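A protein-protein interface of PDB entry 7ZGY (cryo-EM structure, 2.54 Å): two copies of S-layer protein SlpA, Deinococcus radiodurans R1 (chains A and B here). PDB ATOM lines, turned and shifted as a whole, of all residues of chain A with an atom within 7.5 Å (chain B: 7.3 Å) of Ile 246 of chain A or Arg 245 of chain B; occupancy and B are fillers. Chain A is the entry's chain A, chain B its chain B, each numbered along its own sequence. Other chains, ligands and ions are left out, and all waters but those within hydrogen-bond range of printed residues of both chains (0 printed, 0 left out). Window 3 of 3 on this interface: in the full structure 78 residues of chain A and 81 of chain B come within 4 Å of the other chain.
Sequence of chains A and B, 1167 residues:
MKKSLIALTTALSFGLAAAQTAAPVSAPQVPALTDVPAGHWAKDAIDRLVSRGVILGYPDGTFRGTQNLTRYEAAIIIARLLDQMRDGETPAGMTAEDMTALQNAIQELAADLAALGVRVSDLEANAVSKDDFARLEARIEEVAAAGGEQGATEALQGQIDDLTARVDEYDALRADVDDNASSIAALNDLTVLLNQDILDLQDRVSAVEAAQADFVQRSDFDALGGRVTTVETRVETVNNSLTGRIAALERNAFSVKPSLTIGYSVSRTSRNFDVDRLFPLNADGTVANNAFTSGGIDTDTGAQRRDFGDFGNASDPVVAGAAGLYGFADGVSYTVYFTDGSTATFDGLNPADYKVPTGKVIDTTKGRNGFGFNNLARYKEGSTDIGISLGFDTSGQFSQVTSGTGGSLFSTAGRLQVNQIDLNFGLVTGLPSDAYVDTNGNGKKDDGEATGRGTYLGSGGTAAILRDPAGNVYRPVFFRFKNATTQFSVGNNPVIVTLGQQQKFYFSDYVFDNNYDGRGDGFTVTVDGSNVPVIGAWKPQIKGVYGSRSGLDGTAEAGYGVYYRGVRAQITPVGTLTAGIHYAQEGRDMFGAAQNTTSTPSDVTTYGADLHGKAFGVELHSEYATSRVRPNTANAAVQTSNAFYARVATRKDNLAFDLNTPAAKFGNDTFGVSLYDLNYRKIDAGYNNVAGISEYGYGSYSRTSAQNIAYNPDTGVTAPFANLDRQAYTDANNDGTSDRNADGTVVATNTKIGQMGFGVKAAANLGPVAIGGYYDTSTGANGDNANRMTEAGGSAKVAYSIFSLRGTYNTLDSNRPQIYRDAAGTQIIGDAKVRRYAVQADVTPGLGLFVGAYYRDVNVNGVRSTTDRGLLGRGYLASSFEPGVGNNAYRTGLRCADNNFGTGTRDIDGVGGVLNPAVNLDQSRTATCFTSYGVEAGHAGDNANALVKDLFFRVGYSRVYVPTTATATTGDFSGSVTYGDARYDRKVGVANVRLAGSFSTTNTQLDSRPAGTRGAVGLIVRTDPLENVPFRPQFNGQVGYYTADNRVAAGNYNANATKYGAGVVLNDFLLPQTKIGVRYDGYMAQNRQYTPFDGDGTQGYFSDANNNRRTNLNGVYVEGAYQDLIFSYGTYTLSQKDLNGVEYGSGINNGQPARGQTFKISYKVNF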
ATOM      1  N   ASN A 239      21.031  19.757  -0.093  1.00  0.00           N
ATOM      2  CA  ASN A 239      22.096  18.790  -0.320  1.00  0.00           C
ATOM      3  C   ASN A 239      21.567  17.565  -1.050  1.00  0.00           C
ATOM      4  O   ASN A 239      22.182  17.089  -2.009  1.00  0.00           O
ATOM      5  CB  ASN A 239      22.732  18.393   1.011  1.00  0.00           C
ATOM      6  CG  ASN A 239      23.690  17.229   0.876  1.00  0.00           C
ATOM      7  OD1 ASN A 239      24.646  17.282   0.103  1.00  0.00           O
ATOM      8  ND2 ASN A 239      23.439  16.168   1.632  1.00  0.00           N
ATOM      9  N   ASN A 240      20.414  17.050  -0.623  1.00  0.00           N
ATOM     10  CA  ASN A 240      19.878  15.839  -1.232  1.00  0.00           C
ATOM     11  C   ASN A 240      19.440  16.082  -2.671  1.00  0.00           C
ATOM     12  O   ASN A 240      19.733  15.270  -3.555  1.00  0.00           O
ATOM     13  CB  ASN A 240      18.719  15.302  -0.395  1.00  0.00           C
ATOM     14  CG  ASN A 240      19.178  14.733   0.931  1.00  0.00           C
ATOM     15  OD1 ASN A 240      18.680  15.112   1.990  1.00  0.00           O
ATOM     16  ND2 ASN A 240      20.139  13.820   0.880  1.00  0.00           N
ATOM     17  N   SER A 241      18.742  17.189  -2.932  1.00  0.00           N
ATOM     18  CA  SER A 241      18.321  17.469  -4.301  1.00  0.00           C
ATOM     19  C   SER A 241      19.522  17.627  -5.226  1.00  0.00           C
ATOM     20  O   SER A 241      19.554  17.048  -6.323  1.00  0.00           O
ATOM     21  CB  SER A 241      17.451  18.724  -4.339  1.00  0.00           C
ATOM     22  OG  SER A 241      16.423  18.664  -3.368  1.00  0.00           O
ATOM     23  N   LEU A 242      20.524  18.401  -4.804  1.00  0.00           N
ATOM     24  CA  LEU A 242      21.684  18.612  -5.656  1.00  0.00           C
ATOM     25  C   LEU A 242      22.491  17.333  -5.833  1.00  0.00           C
ATOM     26  O   LEU A 242      23.013  17.078  -6.921  1.00  0.00           O
ATOM     27  CB  LEU A 242      22.555  19.732  -5.091  1.00  0.00           C
ATOM     28  CG  LEU A 242      21.878  21.103  -5.075  1.00  0.00           C
ATOM     29  CD1 LEU A 242      22.855  22.191  -4.666  1.00  0.00           C
ATOM     30  CD2 LEU A 242      21.262  21.406  -6.429  1.00  0.00           C
ATOM     31  N   THR A 243      22.602  16.513  -4.787  1.00  0.00           N
ATOM     32  CA  THR A 243      23.292  15.237  -4.926  1.00  0.00           C
ATOM     33  C   THR A 243      22.559  14.319  -5.893  1.00  0.00           C
ATOM     34  O   THR A 243      23.188  13.617  -6.689  1.00  0.00           O
ATOM     35  CB  THR A 243      23.443  14.565  -3.563  1.00  0.00           C
ATOM     36  OG1 THR A 243      24.240  15.392  -2.708  1.00  0.00           O
ATOM     37  CG2 THR A 243      24.107  13.208  -3.709  1.00  0.00           C
ATOM     38  N   GLY A 244      21.227  14.307  -5.841  1.00  0.00           N
ATOM     39  CA  GLY A 244      20.474  13.500  -6.785  1.00  0.00           C
ATOM     40  C   GLY A 244      20.675  13.949  -8.218  1.00  0.00           C
ATOM     41  O   GLY A 244      20.875  13.126  -9.116  1.00  0.00           O
ATOM     42  N   ARG A 245      20.630  15.259  -8.455  1.00  0.00           N
ATOM     43  CA  ARG A 245      20.859  15.748  -9.811  1.00  0.00           C
ATOM     44  C   ARG A 245      22.287  15.490 -10.282  1.00  0.00           C
ATOM     45  O   ARG A 245      22.500  15.157 -11.454  1.00  0.00           O
ATOM     46  CB  ARG A 245      20.516  17.234  -9.902  1.00  0.00           C
ATOM     47  CG  ARG A 245      19.052  17.521  -9.618  1.00  0.00           C
ATOM     48  CD  ARG A 245      18.725  18.998  -9.716  1.00  0.00           C
ATOM     49  NE  ARG A 245      18.673  19.453 -11.100  1.00  0.00           N
ATOM     50  CZ  ARG A 245      18.850  20.711 -11.479  1.00  0.00           C
ATOM     51  NH1 ARG A 245      19.067  21.675 -10.600  1.00  0.00           N
ATOM     52  NH2 ARG A 245      18.799  21.011 -12.774  1.00  0.00           N
ATOM     53  N   ILE A 246      23.271  15.616  -9.390  1.00  0.00           N
ATOM     54  CA  ILE A 246      24.651  15.322  -9.763  1.00  0.00           C
ATOM     55  C   ILE A 246      24.814  13.841 -10.075  1.00  0.00           C
ATOM     56  O   ILE A 246      25.552  13.463 -10.990  1.00  0.00           O
ATOM     57  CB  ILE A 246      25.613  15.776  -8.650  1.00  0.00           C
ATOM     58  CG1 ILE A 246      25.657  17.301  -8.580  1.00  0.00           C
ATOM     59  CG2 ILE A 246      26.998  15.217  -8.892  1.00  0.00           C
ATOM     60  CD1 ILE A 246      26.289  17.833  -7.322  1.00  0.00           C
ATOM     61  N   ALA A 247      24.138  12.977  -9.316  1.00  0.00           N
ATOM     62  CA  ALA A 247      24.189  11.548  -9.599  1.00  0.00           C
ATOM     63  C   ALA A 247      23.555  11.235 -10.946  1.00  0.00           C
ATOM     64  O   ALA A 247      24.058  10.393 -11.696  1.00  0.00           O
ATOM     65  CB  ALA A 247      23.497  10.767  -8.484  1.00  0.00           C
ATOM     66  N   ALA A 248      22.442  11.896 -11.265  1.00  0.00           N
ATOM     67  CA  ALA A 248      21.831  11.701 -12.575  1.00  0.00           C
ATOM     68  C   ALA A 248      22.769  12.149 -13.688  1.00  0.00           C
ATOM     69  O   ALA A 248      22.869  11.490 -14.730  1.00  0.00           O
ATOM     70  CB  ALA A 248      20.502  12.451 -12.652  1.00  0.00           C
ATOM     71  N   LEU A 249      23.462  13.273 -13.491  1.00  0.00           N
ATOM     72  CA  LEU A 249      24.440  13.721 -14.479  1.00  0.00           C
ATOM     73  C   LEU A 249      25.586  12.725 -14.619  1.00  0.00           C
ATOM     74  O   LEU A 249      26.067  12.472 -15.729  1.00  0.00           O
ATOM     75  CB  LEU A 249      24.980  15.101 -14.101  1.00  0.00           C
ATOM     76  CG  LEU A 249      24.188  16.313 -14.590  1.00  0.00           C
ATOM     77  CD1 LEU A 249      24.702  17.578 -13.938  1.00  0.00           C
ATOM     78  CD2 LEU A 249      24.263  16.423 -16.098  1.00  0.00           C
ATOM     79  N   GLU A 250      26.045  12.159 -13.502  1.00  0.00           N
ATOM     80  CA  GLU A 250      27.173  11.235 -13.535  1.00  0.00           C
ATOM     81  C   GLU A 250      26.791   9.885 -14.124  1.00  0.00           C
ATOM     82  O   GLU A 250      27.650   9.179 -14.661  1.00  0.00           O
ATOM     83  CB  GLU A 250      27.735  11.043 -12.128  1.00  0.00           C
ATOM     84  CG  GLU A 250      28.408  12.270 -11.551  1.00  0.00           C
ATOM     85  CD  GLU A 250      28.865  12.060 -10.123  1.00  0.00           C
ATOM     86  OE1 GLU A 250      28.490  11.033  -9.524  1.00  0.00           O
ATOM     87  OE2 GLU A 250      29.605  12.919  -9.601  1.00  0.00           O
ATOM     88  N   ARG A 251      25.517   9.502 -14.024  1.00  0.00           N
ATOM     89  CA  ARG A 251      25.107   8.183 -14.493  1.00  0.00           C
ATOM     90  C   ARG A 251      25.370   8.015 -15.982  1.00  0.00           C
ATOM     91  O   ARG A 251      25.857   6.966 -16.419  1.00  0.00           O
ATOM     92  CB  ARG A 251      23.630   7.948 -14.188  1.00  0.00           C
ATOM     93  CG  ARG A 251      23.143   6.583 -14.624  1.00  0.00           C
ATOM     94  CD  ARG A 251      21.747   6.292 -14.120  1.00  0.00           C
ATOM     95  NE  ARG A 251      21.383   4.899 -14.354  1.00  0.00           N
ATOM     96  CZ  ARG A 251      20.815   4.453 -15.465  1.00  0.00           C
ATOM     97  NH1 ARG A 251      20.517   5.269 -16.463  1.00  0.00           N
ATOM     98  NH2 ARG A 251      20.540   3.157 -15.578  1.00  0.00           N
ATOM     99  N   ASN A 252      25.057   9.029 -16.776  1.00  0.00           N
ATOM    100  CA  ASN A 252      25.175   8.960 -18.225  1.00  0.00           C
ATOM    101  C   ASN A 252      26.172   9.989 -18.740  1.00  0.00           C
ATOM    102  O   ASN A 252      25.923  10.694 -19.720  1.00  0.00           O
ATOM    103  CB  ASN A 252      23.810   9.126 -18.889  1.00  0.00           C
ATOM    104  CG  ASN A 252      23.172  10.459 -18.584  1.00  0.00           C
ATOM    105  OD1 ASN A 252      23.791  11.338 -17.988  1.00  0.00           O
ATOM    106  ND2 ASN A 252      21.916  10.611 -18.978  1.00  0.00           N
ATOM    107  N   ALA A 253      27.317  10.081 -18.074  1.00  0.00           N
ATOM    108  CA  ALA A 253      28.396  10.973 -18.462  1.00  0.00           C
ATOM    109  C   ALA A 253      29.583  10.164 -18.965  1.00  0.00           C
ATOM    110  O   ALA A 253      29.713   8.973 -18.671  1.00  0.00           O
ATOM    111  CB  ALA A 253      28.828  11.857 -17.290  1.00  0.00           C
ATOM    112  N   ASN B 239      28.346  22.608   0.440  1.00  0.00           N
ATOM    113  CA  ASN B 239      28.751  23.424  -0.697  1.00  0.00           C
ATOM    114  C   ASN B 239      30.053  22.915  -1.295  1.00  0.00           C
ATOM    115  O   ASN B 239      30.179  22.786  -2.515  1.00  0.00           O
ATOM    116  CB  ASN B 239      28.886  24.885  -0.268  1.00  0.00           C
ATOM    117  CG  ASN B 239      29.545  25.745  -1.325  1.00  0.00           C
ATOM    118  OD1 ASN B 239      29.080  25.818  -2.462  1.00  0.00           O
ATOM    119  ND2 ASN B 239      30.634  26.405  -0.953  1.00  0.00           N
ATOM    120  N   ASN B 240      31.031  22.600  -0.445  1.00  0.00           N
ATOM    121  CA  ASN B 240      32.330  22.169  -0.945  1.00  0.00           C
ATOM    122  C   ASN B 240      32.249  20.804  -1.616  1.00  0.00           C
ATOM    123  O   ASN B 240      32.826  20.604  -2.690  1.00  0.00           O
ATOM    124  CB  ASN B 240      33.349  22.154   0.193  1.00  0.00           C
ATOM    125  CG  ASN B 240      33.708  23.547   0.666  1.00  0.00           C
ATOM    126  OD1 ASN B 240      33.630  23.852   1.856  1.00  0.00           O
ATOM    127  ND2 ASN B 240      34.097  24.406  -0.268  1.00  0.00           N
ATOM    128  N   SER B 241      31.538  19.851  -1.009  1.00  0.00           N
ATOM    129  CA  SER B 241      31.415  18.538  -1.632  1.00  0.00           C
ATOM    130  C   SER B 241      30.719  18.631  -2.984  1.00  0.00           C
ATOM    131  O   SER B 241      31.179  18.039  -3.973  1.00  0.00           O
ATOM    132  CB  SER B 241      30.658  17.585  -0.708  1.00  0.00           C
ATOM    133  OG  SER B 241      31.187  17.618   0.605  1.00  0.00           O
ATOM    134  N   LEU B 242      29.614  19.376  -3.054  1.00  0.00           N
ATOM    135  CA  LEU B 242      28.891  19.483  -4.314  1.00  0.00           C
ATOM    136  C   LEU B 242      29.695  20.248  -5.357  1.00  0.00           C
ATOM    137  O   LEU B 242      29.654  19.905  -6.541  1.00  0.00           O
ATOM    138  CB  LEU B 242      27.531  20.136  -4.086  1.00  0.00           C
ATOM    139  CG  LEU B 242      26.590  19.314  -3.205  1.00  0.00           C
ATOM    140  CD1 LEU B 242      25.204  19.933  -3.158  1.00  0.00           C
ATOM    141  CD2 LEU B 242      26.528  17.878  -3.691  1.00  0.00           C
ATOM    142  N   THR B 243      30.435  21.279  -4.946  1.00  0.00           N
ATOM    143  CA  THR B 243      31.291  21.988  -5.888  1.00  0.00           C
ATOM    144  C   THR B 243      32.387  21.078  -6.423  1.00  0.00           C
ATOM    145  O   THR B 243      32.721  21.133  -7.609  1.00  0.00           O
ATOM    146  CB  THR B 243      31.897  23.224  -5.224  1.00  0.00           C
ATOM    147  OG1 THR B 243      30.850  24.114  -4.825  1.00  0.00           O
ATOM    148  CG2 THR B 243      32.824  23.941  -6.187  1.00  0.00           C
ATOM    149  N   GLY B 244      32.962  20.237  -5.564  1.00  0.00           N
ATOM    150  CA  GLY B 244      33.966  19.299  -6.036  1.00  0.00           C
ATOM    151  C   GLY B 244      33.408  18.309  -7.039  1.00  0.00           C
ATOM    152  O   GLY B 244      34.025  18.041  -8.074  1.00  0.00           O
ATOM    153  N   ARG B 245      32.231  17.753  -6.750  1.00  0.00           N
ATOM    154  CA  ARG B 245      31.626  16.826  -7.701  1.00  0.00           C
ATOM    155  C   ARG B 245      31.245  17.514  -9.008  1.00  0.00           C
ATOM    156  O   ARG B 245      31.411  16.929 -10.085  1.00  0.00           O
ATOM    157  CB  ARG B 245      30.411  16.144  -7.073  1.00  0.00           C
ATOM    158  CG  ARG B 245      30.765  15.314  -5.852  1.00  0.00           C
ATOM    159  CD  ARG B 245      29.556  14.611  -5.263  1.00  0.00           C
ATOM    160  NE  ARG B 245      29.155  13.459  -6.061  1.00  0.00           N
ATOM    161  CZ  ARG B 245      27.949  12.912  -6.030  1.00  0.00           C
ATOM    162  NH1 ARG B 245      27.003  13.369  -5.227  1.00  0.00           N
ATOM    163  NH2 ARG B 245      27.687  11.871  -6.815  1.00  0.00           N
ATOM    164  N   ILE B 246      30.757  18.753  -8.942  1.00  0.00           N
ATOM    165  CA  ILE B 246      30.422  19.485 -10.160  1.00  0.00           C
ATOM    166  C   ILE B 246      31.679  19.785 -10.965  1.00  0.00           C
ATOM    167  O   ILE B 246      31.667  19.741 -12.198  1.00  0.00           O
ATOM    168  CB  ILE B 246      29.650  20.770  -9.813  1.00  0.00           C
ATOM    169  CG1 ILE B 246      28.256  20.422  -9.293  1.00  0.00           C
ATOM    170  CG2 ILE B 246      29.556  21.673 -11.025  1.00  0.00           C
ATOM    171  CD1 ILE B 246      27.571  21.557  -8.584  1.00  0.00           C
ATOM    172  N   ALA B 247      32.781  20.105 -10.284  1.00  0.00           N
ATOM    173  CA  ALA B 247      34.039  20.339 -10.984  1.00  0.00           C
ATOM    174  C   ALA B 247      34.534  19.069 -11.658  1.00  0.00           C
ATOM    175  O   ALA B 247      35.043  19.111 -12.783  1.00  0.00           O
ATOM    176  CB  ALA B 247      35.087  20.877 -10.014  1.00  0.00           C
ATOM    177  N   ALA B 248      34.406  17.928 -10.980  1.00  0.00           N
ATOM    178  CA  ALA B 248      34.786  16.665 -11.602  1.00  0.00           C
ATOM    179  C   ALA B 248      33.926  16.375 -12.826  1.00  0.00           C
ATOM    180  O   ALA B 248      34.426  15.877 -13.840  1.00  0.00           O
ATOM    181  CB  ALA B 248      34.687  15.527 -10.588  1.00  0.00           C
ATOM    182  N   LEU B 249      32.626  16.670 -12.746  1.00  0.00           N
ATOM    183  CA  LEU B 249      31.759  16.507 -13.910  1.00  0.00           C
ATOM    184  C   LEU B 249      32.172  17.436 -15.047  1.00  0.00           C
ATOM    185  O   LEU B 249      32.157  17.042 -16.218  1.00  0.00           O
ATOM    186  CB  LEU B 249      30.301  16.758 -13.525  1.00  0.00           C
ATOM    187  CG  LEU B 249      29.509  15.563 -12.998  1.00  0.00           C
ATOM    188  CD1 LEU B 249      28.174  16.015 -12.445  1.00  0.00           C
ATOM    189  CD2 LEU B 249      29.313  14.531 -14.087  1.00  0.00           C
ATOM    190  N   GLU B 250      32.529  18.679 -14.722  1.00  0.00           N
ATOM    191  CA  GLU B 250      32.875  19.657 -15.747  1.00  0.00           C
ATOM    192  C   GLU B 250      34.230  19.371 -16.377  1.00  0.00           C
ATOM    193  O   GLU B 250      34.472  19.765 -17.523  1.00  0.00           O
ATOM    194  CB  GLU B 250      32.866  21.062 -15.151  1.00  0.00           C
ATOM    195  CG  GLU B 250      31.494  21.565 -14.758  1.00  0.00           C
ATOM    196  CD  GLU B 250      31.539  22.938 -14.123  1.00  0.00           C
ATOM    197  OE1 GLU B 250      32.652  23.418 -13.827  1.00  0.00           O
ATOM    198  OE2 GLU B 250      30.464  23.539 -13.925  1.00  0.00           O
ATOM    199  N   ARG B 251      35.125  18.705 -15.649  1.00  0.00           N
ATOM    200  CA  ARG B 251      36.464  18.465 -16.177  1.00  0.00           C
ATOM    201  C   ARG B 251      36.419  17.643 -17.457  1.00  0.00           C
ATOM    202  O   ARG B 251      37.138  17.939 -18.417  1.00  0.00           O
ATOM    203  CB  ARG B 251      37.329  17.769 -15.129  1.00  0.00           C
ATOM    204  CG  ARG B 251      38.748  17.530 -15.594  1.00  0.00           C
ATOM    205  CD  ARG B 251      39.644  17.059 -14.467  1.00  0.00           C
ATOM    206  NE  ARG B 251      41.044  17.069 -14.869  1.00  0.00           N
ATOM    207  CZ  ARG B 251      41.658  16.055 -15.460  1.00  0.00           C
ATOM    208  NH1 ARG B 251      41.025  14.922 -15.721  1.00  0.00           N
ATOM    209  NH2 ARG B 251      42.937  16.179 -15.799  1.00  0.00           N
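The side-chain carboxylate (OE1) of Glu 250 of chain A is in salt-bridge range of the guanidinium group (NH2) of Arg 245 of chain B, 2.9 Å away.
The backbone carbonyl oxygen (O) of Asn 239 of chain A sits at hydrogen-bond distance from the side-chain hydroxyl (OG1) of Thr 243 of chain A (2.8 Å). The backbone carbonyl oxygen (O) of Leu 249 of chain A sits close to the side-chain amide oxygen (OD1) of Asn 252 of chain A.
Leu 242 of chain A touches Leu 242 of chain B. Leu 242 of chain B touches Thr 243 of chain A (CD2 to OG1, 3.5 Å). Arg 245 of chain B touches Thr 243 of chain A. CD1 of Ile 246 of chain A touches CD2 of Leu 242 of chain B, at 3.6 Å. Ile 246 of chain A touches Arg 245 of chain B. CD1 of Ile 246 of chain A touches CG1 of Ile 246 of chain B (3.8 Å). Ile 246 of chain A touches Leu 249 of chain B (CG2 to CD1, 3.8 Å). Leu 249 of chain A touches Leu 249 of chain B (CB to CD1, 3.7 Å). CG of Glu 250 of chain A touches CD2 of Leu 249 of chain B, 3.5 Å away.
Of the printed residues of chain B, Thr 243 of chain A touches Leu 242 (3.5 Å) and Arg 245 (3.3 Å). Printed residues of chain B within 4 Å of Glu 250 of chain A: Arg 245 and Leu 249. Of the printed residues of chain A, Leu 242 of chain B touches Leu 242, Thr 243 and Ile 246. Gly 244 of chain B touches none of the printed residues of chain A. Of chain A, only Thr 243 (3.3 Å), Ile 246 (3.8 Å) and Glu 250 (2.9 Å) come within 4 Å of Arg 245 of chain B. Of the printed residues of chain A, Ile 246 of chain B touches Ile 246 (3.8 Å). The nearest residue of chain B that does not touch Ile 246 of chain A is Thr 243 of chain B (5.9 Å). The nearest printed residue of chain A that does not touch Leu 242 of chain B is Asn 239 of chain A (4.2 Å).
Of the 13 printed residues of chain B, 4 touch a printed residue of chain A. Hydrophobic or aromatic side chains of chain B within 4 Å of the printed part of chain A: Leu 242, Ile 246 and Leu 249. Printed residues of chain A that touch a printed residue of chain B: Leu 242, Thr 243, Ile 246, Leu 249 and Glu 250. Among the printed residues, 10 pairs touch across the chains.
Leu 242 of chain B touches its own counterpart, Leu 242 of chain A. Thr 243 of chain A touches Arg 245 of chain B, but with the chains exchanged Arg 245 of chain A does not touch Thr 243 of chain B (11.3 Å). Ile 246 of chain A touches Leu 242 of chain B, but with the chains exchanged Leu 242 of chain A does not touch Ile 246 of chain B (6.2 Å). Ile 246 of chain A touches its own counterpart, Ile 246 of chain B. Positions printed for both chains: 239, 240, 241, 242, 243, 244, 245, 246, 247, 248, 249, 250 and 251. Of the 10 pairs that touch across the chains among the printed residues, 3 have their exchanged pair printed and touching as well.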
